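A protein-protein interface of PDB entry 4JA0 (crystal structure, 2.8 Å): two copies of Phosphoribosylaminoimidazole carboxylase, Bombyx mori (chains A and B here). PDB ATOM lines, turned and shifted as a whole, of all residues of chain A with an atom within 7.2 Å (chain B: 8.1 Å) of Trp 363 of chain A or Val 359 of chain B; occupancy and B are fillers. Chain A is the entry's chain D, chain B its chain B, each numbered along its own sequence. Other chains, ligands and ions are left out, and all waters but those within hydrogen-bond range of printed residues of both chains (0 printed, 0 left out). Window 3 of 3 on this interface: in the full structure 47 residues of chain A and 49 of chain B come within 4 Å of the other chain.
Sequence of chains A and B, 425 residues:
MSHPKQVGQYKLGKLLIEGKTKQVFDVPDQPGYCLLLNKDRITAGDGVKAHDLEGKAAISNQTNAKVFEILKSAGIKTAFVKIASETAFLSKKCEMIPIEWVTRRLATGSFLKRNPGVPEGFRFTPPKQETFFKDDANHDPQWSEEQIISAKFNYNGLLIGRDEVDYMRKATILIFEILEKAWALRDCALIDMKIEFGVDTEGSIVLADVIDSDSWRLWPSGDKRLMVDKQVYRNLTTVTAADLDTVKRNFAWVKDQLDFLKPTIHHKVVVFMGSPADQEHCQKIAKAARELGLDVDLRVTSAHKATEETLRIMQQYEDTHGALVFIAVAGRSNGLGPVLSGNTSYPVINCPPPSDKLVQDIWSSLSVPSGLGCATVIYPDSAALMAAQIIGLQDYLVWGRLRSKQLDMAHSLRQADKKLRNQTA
Of the 13 printed residues of chain B, 5 touch a printed residue of chain A.
Among the printed residues, 7 pairs touch across the chains.
Ile 362 of chain A touches Leu 366 of chain B, and with the chains exchanged Leu 366 of chain A touches Ile 362 of chain B.
Trp 363 of chain A touches Val 359 of chain B, but with the chains exchanged Val 359 of chain A does not touch Trp 363 of chain B (4.1 Å).
Positions printed for both chains: 358, 359, 360, 361, 362, 363, 364 and 366.
Trp 363 of chain A touches two residues of chain B.
Printed residues of chain B within 4 Å of Val 368 of chain A: Tyr 379.
Printed residues of chain A within 4 Å of Ile 378 of chain B: Trp 363 and Leu 366.
Printed residues of chain B within 4 Å of Leu 366 of chain A: Ile 362 and Ile 378.
Printed residues of chain A within 4 Å of Tyr 379 of chain B: Ser 367 and Val 368.
Printed residues of chain B within 4 Å of Ser 367 of chain A: Tyr 379.
The nearest printed residue of chain B that does not touch Ile 362 of chain A is Trp 363 of chain B (4.02 Å).
The backbone carbonyl oxygen of Trp 363 of chain A is in hydrogen-bond range of the side-chain hydroxyl of Ser 367 of chain A, at 2.5 Å.
Leu 366 of chain B touches Ile 362 of chain A.
Trp 363 of chain A touches Val 359 of chain B (CZ2 to CA, 3.96 Å).
Trp 363 of chain A touches Ile 378 of chain B (CZ3 to CD1, 3.6 Å).
Leu 366 of chain A touches Ile 362 of chain B.
Ile 378 of chain B touches Leu 366 of chain A (CD1 to CB, 3.6 Å).
CB of Ser 367 of chain A touches OH of Tyr 379 of chain B, 3.3 Å away.
Tyr 379 of chain B touches Val 368 of chain A (CE2 to O, 3.5 Å).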
ATOM      1  N   ASN A 334     -34.196 -23.118  20.555  1.00  0.00           N
ATOM      2  CA  ASN A 334     -34.510 -24.314  21.304  1.00  0.00           C
ATOM      3  C   ASN A 334     -34.463 -24.080  22.807  1.00  0.00           C
ATOM      4  O   ASN A 334     -33.385 -24.094  23.420  1.00  0.00           O
ATOM      5  CB  ASN A 334     -33.545 -25.430  20.896  1.00  0.00           C
ATOM      6  CG  ASN A 334     -33.590 -26.617  21.827  1.00  0.00           C
ATOM      7  OD1 ASN A 334     -34.647 -26.954  22.402  1.00  0.00           O
ATOM      8  ND2 ASN A 334     -32.449 -27.296  21.952  1.00  0.00           N
ATOM      9  N   LEU A 358     -30.232 -23.436  10.910  1.00  0.00           N
ATOM     10  CA  LEU A 358     -29.543 -24.237  11.927  1.00  0.00           C
ATOM     11  C   LEU A 358     -28.141 -23.694  12.248  1.00  0.00           C
ATOM     12  O   LEU A 358     -27.674 -23.796  13.380  1.00  0.00           O
ATOM     13  CB  LEU A 358     -29.463 -25.715  11.513  1.00  0.00           C
ATOM     14  CG  LEU A 358     -28.801 -26.748  12.467  1.00  0.00           C
ATOM     15  CD1 LEU A 358     -29.536 -26.848  13.805  1.00  0.00           C
ATOM     16  CD2 LEU A 358     -28.670 -28.147  11.862  1.00  0.00           C
ATOM     17  N   VAL A 359     -27.487 -23.089  11.262  1.00  0.00           N
ATOM     18  CA  VAL A 359     -26.181 -22.471  11.484  1.00  0.00           C
ATOM     19  C   VAL A 359     -26.239 -21.350  12.523  1.00  0.00           C
ATOM     20  O   VAL A 359     -25.279 -21.165  13.274  1.00  0.00           O
ATOM     21  CB  VAL A 359     -25.599 -21.911  10.171  1.00  0.00           C
ATOM     22  CG1 VAL A 359     -24.170 -21.442  10.382  1.00  0.00           C
ATOM     23  CG2 VAL A 359     -25.641 -22.983   9.110  1.00  0.00           C
ATOM     24  N   GLN A 360     -27.357 -20.616  12.569  1.00  0.00           N
ATOM     25  CA  GLN A 360     -27.575 -19.585  13.596  1.00  0.00           C
ATOM     26  C   GLN A 360     -28.229 -20.209  14.845  1.00  0.00           C
ATOM     27  O   GLN A 360     -27.842 -19.915  15.974  1.00  0.00           O
ATOM     28  CB  GLN A 360     -28.475 -18.458  13.078  1.00  0.00           C
ATOM     29  CG  GLN A 360     -27.822 -17.475  12.118  1.00  0.00           C
ATOM     30  CD  GLN A 360     -27.587 -18.073  10.740  1.00  0.00           C
ATOM     31  OE1 GLN A 360     -28.481 -18.710  10.162  1.00  0.00           O
ATOM     32  NE2 GLN A 360     -26.403 -17.837  10.185  1.00  0.00           N
ATOM     33  N   ASP A 361     -29.213 -21.078  14.630  1.00  0.00           N
ATOM     34  CA  ASP A 361     -30.039 -21.603  15.713  1.00  0.00           C
ATOM     35  C   ASP A 361     -29.328 -22.574  16.654  1.00  0.00           C
ATOM     36  O   ASP A 361     -29.767 -22.795  17.778  1.00  0.00           O
ATOM     37  CB  ASP A 361     -31.291 -22.312  15.156  1.00  0.00           C
ATOM     38  CG  ASP A 361     -32.370 -21.341  14.648  1.00  0.00           C
ATOM     39  OD1 ASP A 361     -32.365 -20.146  15.049  1.00  0.00           O
ATOM     40  OD2 ASP A 361     -33.258 -21.805  13.878  1.00  0.00           O
ATOM     41  N   ILE A 362     -28.229 -23.169  16.218  1.00  0.00           N
ATOM     42  CA  ILE A 362     -27.642 -24.236  17.019  1.00  0.00           C
ATOM     43  C   ILE A 362     -27.050 -23.781  18.354  1.00  0.00           C
ATOM     44  O   ILE A 362     -26.805 -24.593  19.250  1.00  0.00           O
ATOM     45  CB  ILE A 362     -26.590 -25.032  16.246  1.00  0.00           C
ATOM     46  CG1 ILE A 362     -26.507 -26.431  16.866  1.00  0.00           C
ATOM     47  CG2 ILE A 362     -25.274 -24.270  16.198  1.00  0.00           C
ATOM     48  CD1 ILE A 362     -25.464 -27.247  16.346  1.00  0.00           C
ATOM     49  N   TRP A 363     -26.795 -22.488  18.492  1.00  0.00           N
ATOM     50  CA  TRP A 363     -26.218 -22.010  19.731  1.00  0.00           C
ATOM     51  C   TRP A 363     -27.240 -21.952  20.858  1.00  0.00           C
ATOM     52  O   TRP A 363     -26.868 -21.827  22.013  1.00  0.00           O
ATOM     53  CB  TRP A 363     -25.557 -20.652  19.512  1.00  0.00           C
ATOM     54  CG  TRP A 363     -24.395 -20.763  18.620  1.00  0.00           C
ATOM     55  CD1 TRP A 363     -24.383 -20.582  17.280  1.00  0.00           C
ATOM     56  CD2 TRP A 363     -23.062 -21.118  18.991  1.00  0.00           C
ATOM     57  NE1 TRP A 363     -23.123 -20.792  16.786  1.00  0.00           N
ATOM     58  CE2 TRP A 363     -22.292 -21.122  17.818  1.00  0.00           C
ATOM     59  CE3 TRP A 363     -22.446 -21.423  20.200  1.00  0.00           C
ATOM     60  CZ2 TRP A 363     -20.939 -21.417  17.816  1.00  0.00           C
ATOM     61  CZ3 TRP A 363     -21.101 -21.729  20.195  1.00  0.00           C
ATOM     62  CH2 TRP A 363     -20.361 -21.729  19.012  1.00  0.00           C
ATOM     63  N   SER A 364     -28.522 -22.084  20.535  1.00  0.00           N
ATOM     64  CA  SER A 364     -29.544 -22.094  21.576  1.00  0.00           C
ATOM     65  C   SER A 364     -29.541 -23.449  22.267  1.00  0.00           C
ATOM     66  O   SER A 364     -29.981 -23.552  23.413  1.00  0.00           O
ATOM     67  CB  SER A 364     -30.921 -21.780  21.010  1.00  0.00           C
ATOM     68  OG  SER A 364     -31.293 -22.726  20.037  1.00  0.00           O
ATOM     69  N   SER A 365     -29.034 -24.465  21.553  1.00  0.00           N
ATOM     70  CA  SER A 365     -28.865 -25.836  22.050  1.00  0.00           C
ATOM     71  C   SER A 365     -27.563 -25.973  22.816  1.00  0.00           C
ATOM     72  O   SER A 365     -27.548 -26.396  23.969  1.00  0.00           O
ATOM     73  CB  SER A 365     -28.878 -26.852  20.902  1.00  0.00           C
ATOM     74  OG  SER A 365     -30.151 -26.957  20.292  1.00  0.00           O
ATOM     75  N   LEU A 366     -26.458 -25.630  22.167  1.00  0.00           N
ATOM     76  CA  LEU A 366     -25.178 -25.492  22.859  1.00  0.00           C
ATOM     77  C   LEU A 366     -25.337 -24.298  23.785  1.00  0.00           C
ATOM     78  O   LEU A 366     -26.392 -23.670  23.799  1.00  0.00           O
ATOM     79  CB  LEU A 366     -24.067 -25.208  21.845  1.00  0.00           C
ATOM     80  CG  LEU A 366     -24.007 -26.133  20.623  1.00  0.00           C
ATOM     81  CD1 LEU A 366     -23.190 -25.482  19.521  1.00  0.00           C
ATOM     82  CD2 LEU A 366     -23.463 -27.504  20.985  1.00  0.00           C
ATOM     83  N   SER A 367     -24.322 -23.984  24.572  1.00  0.00           N
ATOM     84  CA  SER A 367     -24.343 -22.732  25.374  1.00  0.00           C
ATOM     85  C   SER A 367     -25.614 -22.600  26.183  1.00  0.00           C
ATOM     86  O   SER A 367     -26.347 -21.623  26.080  1.00  0.00           O
ATOM     87  CB  SER A 367     -24.096 -21.433  24.553  1.00  0.00           C
ATOM     88  OG  SER A 367     -25.100 -21.165  23.601  1.00  0.00           O
ATOM     89  N   VAL A 368     -25.829 -23.616  27.000  1.00  0.00           N
ATOM     90  CA  VAL A 368     -26.889 -23.649  27.961  1.00  0.00           C
ATOM     91  C   VAL A 368     -26.360 -22.922  29.184  1.00  0.00           C
ATOM     92  O   VAL A 368     -25.165 -22.705  29.305  1.00  0.00           O
ATOM     93  CB  VAL A 368     -27.168 -25.096  28.319  1.00  0.00           C
ATOM     94  CG1 VAL A 368     -27.851 -25.792  27.169  1.00  0.00           C
ATOM     95  CG2 VAL A 368     -25.863 -25.779  28.646  1.00  0.00           C
ATOM     96  N   SER B 355     -12.010 -21.083  23.635  1.00  0.00           N
ATOM     97  CA  SER B 355     -11.150 -20.493  22.609  1.00  0.00           C
ATOM     98  C   SER B 355     -11.945 -19.502  21.740  1.00  0.00           C
ATOM     99  O   SER B 355     -13.152 -19.671  21.523  1.00  0.00           O
ATOM    100  CB  SER B 355     -10.554 -21.619  21.746  1.00  0.00           C
ATOM    101  OG  SER B 355     -10.023 -21.151  20.523  1.00  0.00           O
ATOM    102  N   ASP B 356     -11.257 -18.497  21.201  1.00  0.00           N
ATOM    103  CA  ASP B 356     -11.904 -17.537  20.314  1.00  0.00           C
ATOM    104  C   ASP B 356     -12.359 -18.239  19.046  1.00  0.00           C
ATOM    105  O   ASP B 356     -13.402 -17.920  18.469  1.00  0.00           O
ATOM    106  CB  ASP B 356     -10.931 -16.409  19.968  1.00  0.00           C
ATOM    107  CG  ASP B 356     -10.678 -15.477  21.142  1.00  0.00           C
ATOM    108  OD1 ASP B 356     -11.581 -15.364  21.997  1.00  0.00           O
ATOM    109  OD2 ASP B 356      -9.594 -14.857  21.209  1.00  0.00           O
ATOM    110  N   LYS B 357     -11.595 -19.240  18.653  1.00  0.00           N
ATOM    111  CA  LYS B 357     -11.869 -19.954  17.434  1.00  0.00           C
ATOM    112  C   LYS B 357     -13.000 -20.986  17.585  1.00  0.00           C
ATOM    113  O   LYS B 357     -13.409 -21.600  16.593  1.00  0.00           O
ATOM    114  CB  LYS B 357     -10.587 -20.637  16.944  1.00  0.00           C
ATOM    115  CG  LYS B 357      -9.619 -19.732  16.185  1.00  0.00           C
ATOM    116  CD  LYS B 357      -8.465 -19.286  17.089  1.00  0.00           C
ATOM    117  CE  LYS B 357      -7.344 -18.554  16.314  1.00  0.00           C
ATOM    118  NZ  LYS B 357      -6.022 -18.502  17.046  1.00  0.00           N
ATOM    119  N   LEU B 358     -13.528 -21.159  18.800  1.00  0.00           N
ATOM    120  CA  LEU B 358     -14.538 -22.196  19.030  1.00  0.00           C
ATOM    121  C   LEU B 358     -15.768 -22.030  18.136  1.00  0.00           C
ATOM    122  O   LEU B 358     -16.369 -23.017  17.710  1.00  0.00           O
ATOM    123  CB  LEU B 358     -14.948 -22.233  20.495  1.00  0.00           C
ATOM    124  CG  LEU B 358     -16.004 -23.272  20.909  1.00  0.00           C
ATOM    125  CD1 LEU B 358     -15.536 -24.703  20.649  1.00  0.00           C
ATOM    126  CD2 LEU B 358     -16.333 -23.105  22.374  1.00  0.00           C
ATOM    127  N   VAL B 359     -16.112 -20.781  17.824  1.00  0.00           N
ATOM    128  CA  VAL B 359     -17.202 -20.490  16.898  1.00  0.00           C
ATOM    129  C   VAL B 359     -16.960 -21.110  15.519  1.00  0.00           C
ATOM    130  O   VAL B 359     -17.899 -21.496  14.825  1.00  0.00           O
ATOM    131  CB  VAL B 359     -17.390 -18.975  16.733  1.00  0.00           C
ATOM    132  CG1 VAL B 359     -18.550 -18.675  15.807  1.00  0.00           C
ATOM    133  CG2 VAL B 359     -17.572 -18.337  18.066  1.00  0.00           C
ATOM    134  N   GLN B 360     -15.700 -21.187  15.112  1.00  0.00           N
ATOM    135  CA  GLN B 360     -15.379 -21.826  13.854  1.00  0.00           C
ATOM    136  C   GLN B 360     -15.117 -23.319  14.071  1.00  0.00           C
ATOM    137  O   GLN B 360     -15.650 -24.159  13.337  1.00  0.00           O
ATOM    138  CB  GLN B 360     -14.154 -21.176  13.215  1.00  0.00           C
ATOM    139  CG  GLN B 360     -14.433 -19.873  12.551  1.00  0.00           C
ATOM    140  CD  GLN B 360     -14.706 -18.765  13.542  1.00  0.00           C
ATOM    141  OE1 GLN B 360     -13.963 -18.573  14.506  1.00  0.00           O
ATOM    142  NE2 GLN B 360     -15.769 -18.012  13.297  1.00  0.00           N
ATOM    143  N   ASP B 361     -14.339 -23.644  15.104  1.00  0.00           N
ATOM    144  CA  ASP B 361     -13.850 -25.004  15.290  1.00  0.00           C
ATOM    145  C   ASP B 361     -14.931 -25.996  15.685  1.00  0.00           C
ATOM    146  O   ASP B 361     -14.758 -27.207  15.518  1.00  0.00           O
ATOM    147  CB  ASP B 361     -12.746 -25.050  16.344  1.00  0.00           C
ATOM    148  CG  ASP B 361     -11.433 -24.471  15.857  1.00  0.00           C
ATOM    149  OD1 ASP B 361     -11.227 -24.383  14.613  1.00  0.00           O
ATOM    150  OD2 ASP B 361     -10.598 -24.130  16.733  1.00  0.00           O
ATOM    151  N   ILE B 362     -16.054 -25.497  16.190  1.00  0.00           N
ATOM    152  CA  ILE B 362     -17.030 -26.398  16.757  1.00  0.00           C
ATOM    153  C   ILE B 362     -17.697 -27.320  15.760  1.00  0.00           C
ATOM    154  O   ILE B 362     -18.137 -28.420  16.115  1.00  0.00           O
ATOM    155  CB  ILE B 362     -18.125 -25.666  17.544  1.00  0.00           C
ATOM    156  CG1 ILE B 362     -18.746 -26.665  18.523  1.00  0.00           C
ATOM    157  CG2 ILE B 362     -19.148 -25.005  16.586  1.00  0.00           C
ATOM    158  CD1 ILE B 362     -19.874 -26.172  19.239  1.00  0.00           C
ATOM    159  N   TRP B 363     -17.721 -26.936  14.501  1.00  0.00           N
ATOM    160  CA  TRP B 363     -18.371 -27.796  13.537  1.00  0.00           C
ATOM    161  C   TRP B 363     -17.534 -29.040  13.253  1.00  0.00           C
ATOM    162  O   TRP B 363     -18.012 -29.966  12.616  1.00  0.00           O
ATOM    163  CB  TRP B 363     -18.660 -27.029  12.265  1.00  0.00           C
ATOM    164  CG  TRP B 363     -19.610 -25.944  12.521  1.00  0.00           C
ATOM    165  CD1 TRP B 363     -19.312 -24.654  12.807  1.00  0.00           C
ATOM    166  CD2 TRP B 363     -21.038 -26.043  12.526  1.00  0.00           C
ATOM    167  NE1 TRP B 363     -20.472 -23.931  12.992  1.00  0.00           N
ATOM    168  CE2 TRP B 363     -21.544 -24.760  12.817  1.00  0.00           C
ATOM    169  CE3 TRP B 363     -21.937 -27.090  12.304  1.00  0.00           C
ATOM    170  CZ2 TRP B 363     -22.906 -24.496  12.905  1.00  0.00           C
ATOM    171  CZ3 TRP B 363     -23.296 -26.828  12.393  1.00  0.00           C
ATOM    172  CH2 TRP B 363     -23.768 -25.545  12.693  1.00  0.00           C
ATOM    173  N   SER B 364     -16.300 -29.093  13.740  1.00  0.00           N
ATOM    174  CA  SER B 364     -15.539 -30.321  13.561  1.00  0.00           C
ATOM    175  C   SER B 364     -16.038 -31.377  14.540  1.00  0.00           C
ATOM    176  O   SER B 364     -15.883 -32.577  14.279  1.00  0.00           O
ATOM    177  CB  SER B 364     -14.036 -30.074  13.712  1.00  0.00           C
ATOM    178  OG  SER B 364     -13.733 -29.491  14.962  1.00  0.00           O
ATOM    179  N   LEU B 366     -19.483 -31.174  16.019  1.00  0.00           N
ATOM    180  CA  LEU B 366     -20.779 -31.412  15.403  1.00  0.00           C
ATOM    181  C   LEU B 366     -20.505 -31.936  14.000  1.00  0.00           C
ATOM    182  O   LEU B 366     -19.356 -31.920  13.554  1.00  0.00           O
ATOM    183  CB  LEU B 366     -21.536 -30.098  15.280  1.00  0.00           C
ATOM    184  CG  LEU B 366     -21.671 -29.219  16.509  1.00  0.00           C
ATOM    185  CD1 LEU B 366     -22.028 -27.825  16.067  1.00  0.00           C
ATOM    186  CD2 LEU B 366     -22.755 -29.792  17.379  1.00  0.00           C
ATOM    187  N   ILE B 378     -20.184 -27.824  25.413  1.00  0.00           N
ATOM    188  CA  ILE B 378     -19.263 -26.688  25.271  1.00  0.00           C
ATOM    189  C   ILE B 378     -18.613 -26.203  26.582  1.00  0.00           C
ATOM    190  O   ILE B 378     -17.601 -25.486  26.581  1.00  0.00           O
ATOM    191  CB  ILE B 378     -19.996 -25.575  24.533  1.00  0.00           C
ATOM    192  CG1 ILE B 378     -19.771 -25.730  23.041  1.00  0.00           C
ATOM    193  CG2 ILE B 378     -19.637 -24.170  25.027  1.00  0.00           C
ATOM    194  CD1 ILE B 378     -20.517 -24.657  22.276  1.00  0.00           C
ATOM    195  N   TYR B 379     -19.189 -26.614  27.705  1.00  0.00           N
ATOM    196  CA  TYR B 379     -18.657 -26.226  28.999  1.00  0.00           C
ATOM    197  C   TYR B 379     -18.202 -27.443  29.770  1.00  0.00           C
ATOM    198  O   TYR B 379     -18.838 -28.498  29.702  1.00  0.00           O
ATOM    199  CB  TYR B 379     -19.705 -25.445  29.790  1.00  0.00           C
ATOM    200  CG  TYR B 379     -20.295 -24.287  29.005  1.00  0.00           C
ATOM    201  CD1 TYR B 379     -19.566 -23.124  28.824  1.00  0.00           C
ATOM    202  CD2 TYR B 379     -21.570 -24.357  28.450  1.00  0.00           C
ATOM    203  CE1 TYR B 379     -20.068 -22.077  28.107  1.00  0.00           C
ATOM    204  CE2 TYR B 379     -22.080 -23.305  27.735  1.00  0.00           C
ATOM    205  CZ  TYR B 379     -21.322 -22.162  27.567  1.00  0.00           C
ATOM    206  OH  TYR B 379     -21.794 -21.075  26.860  1.00  0.00           O
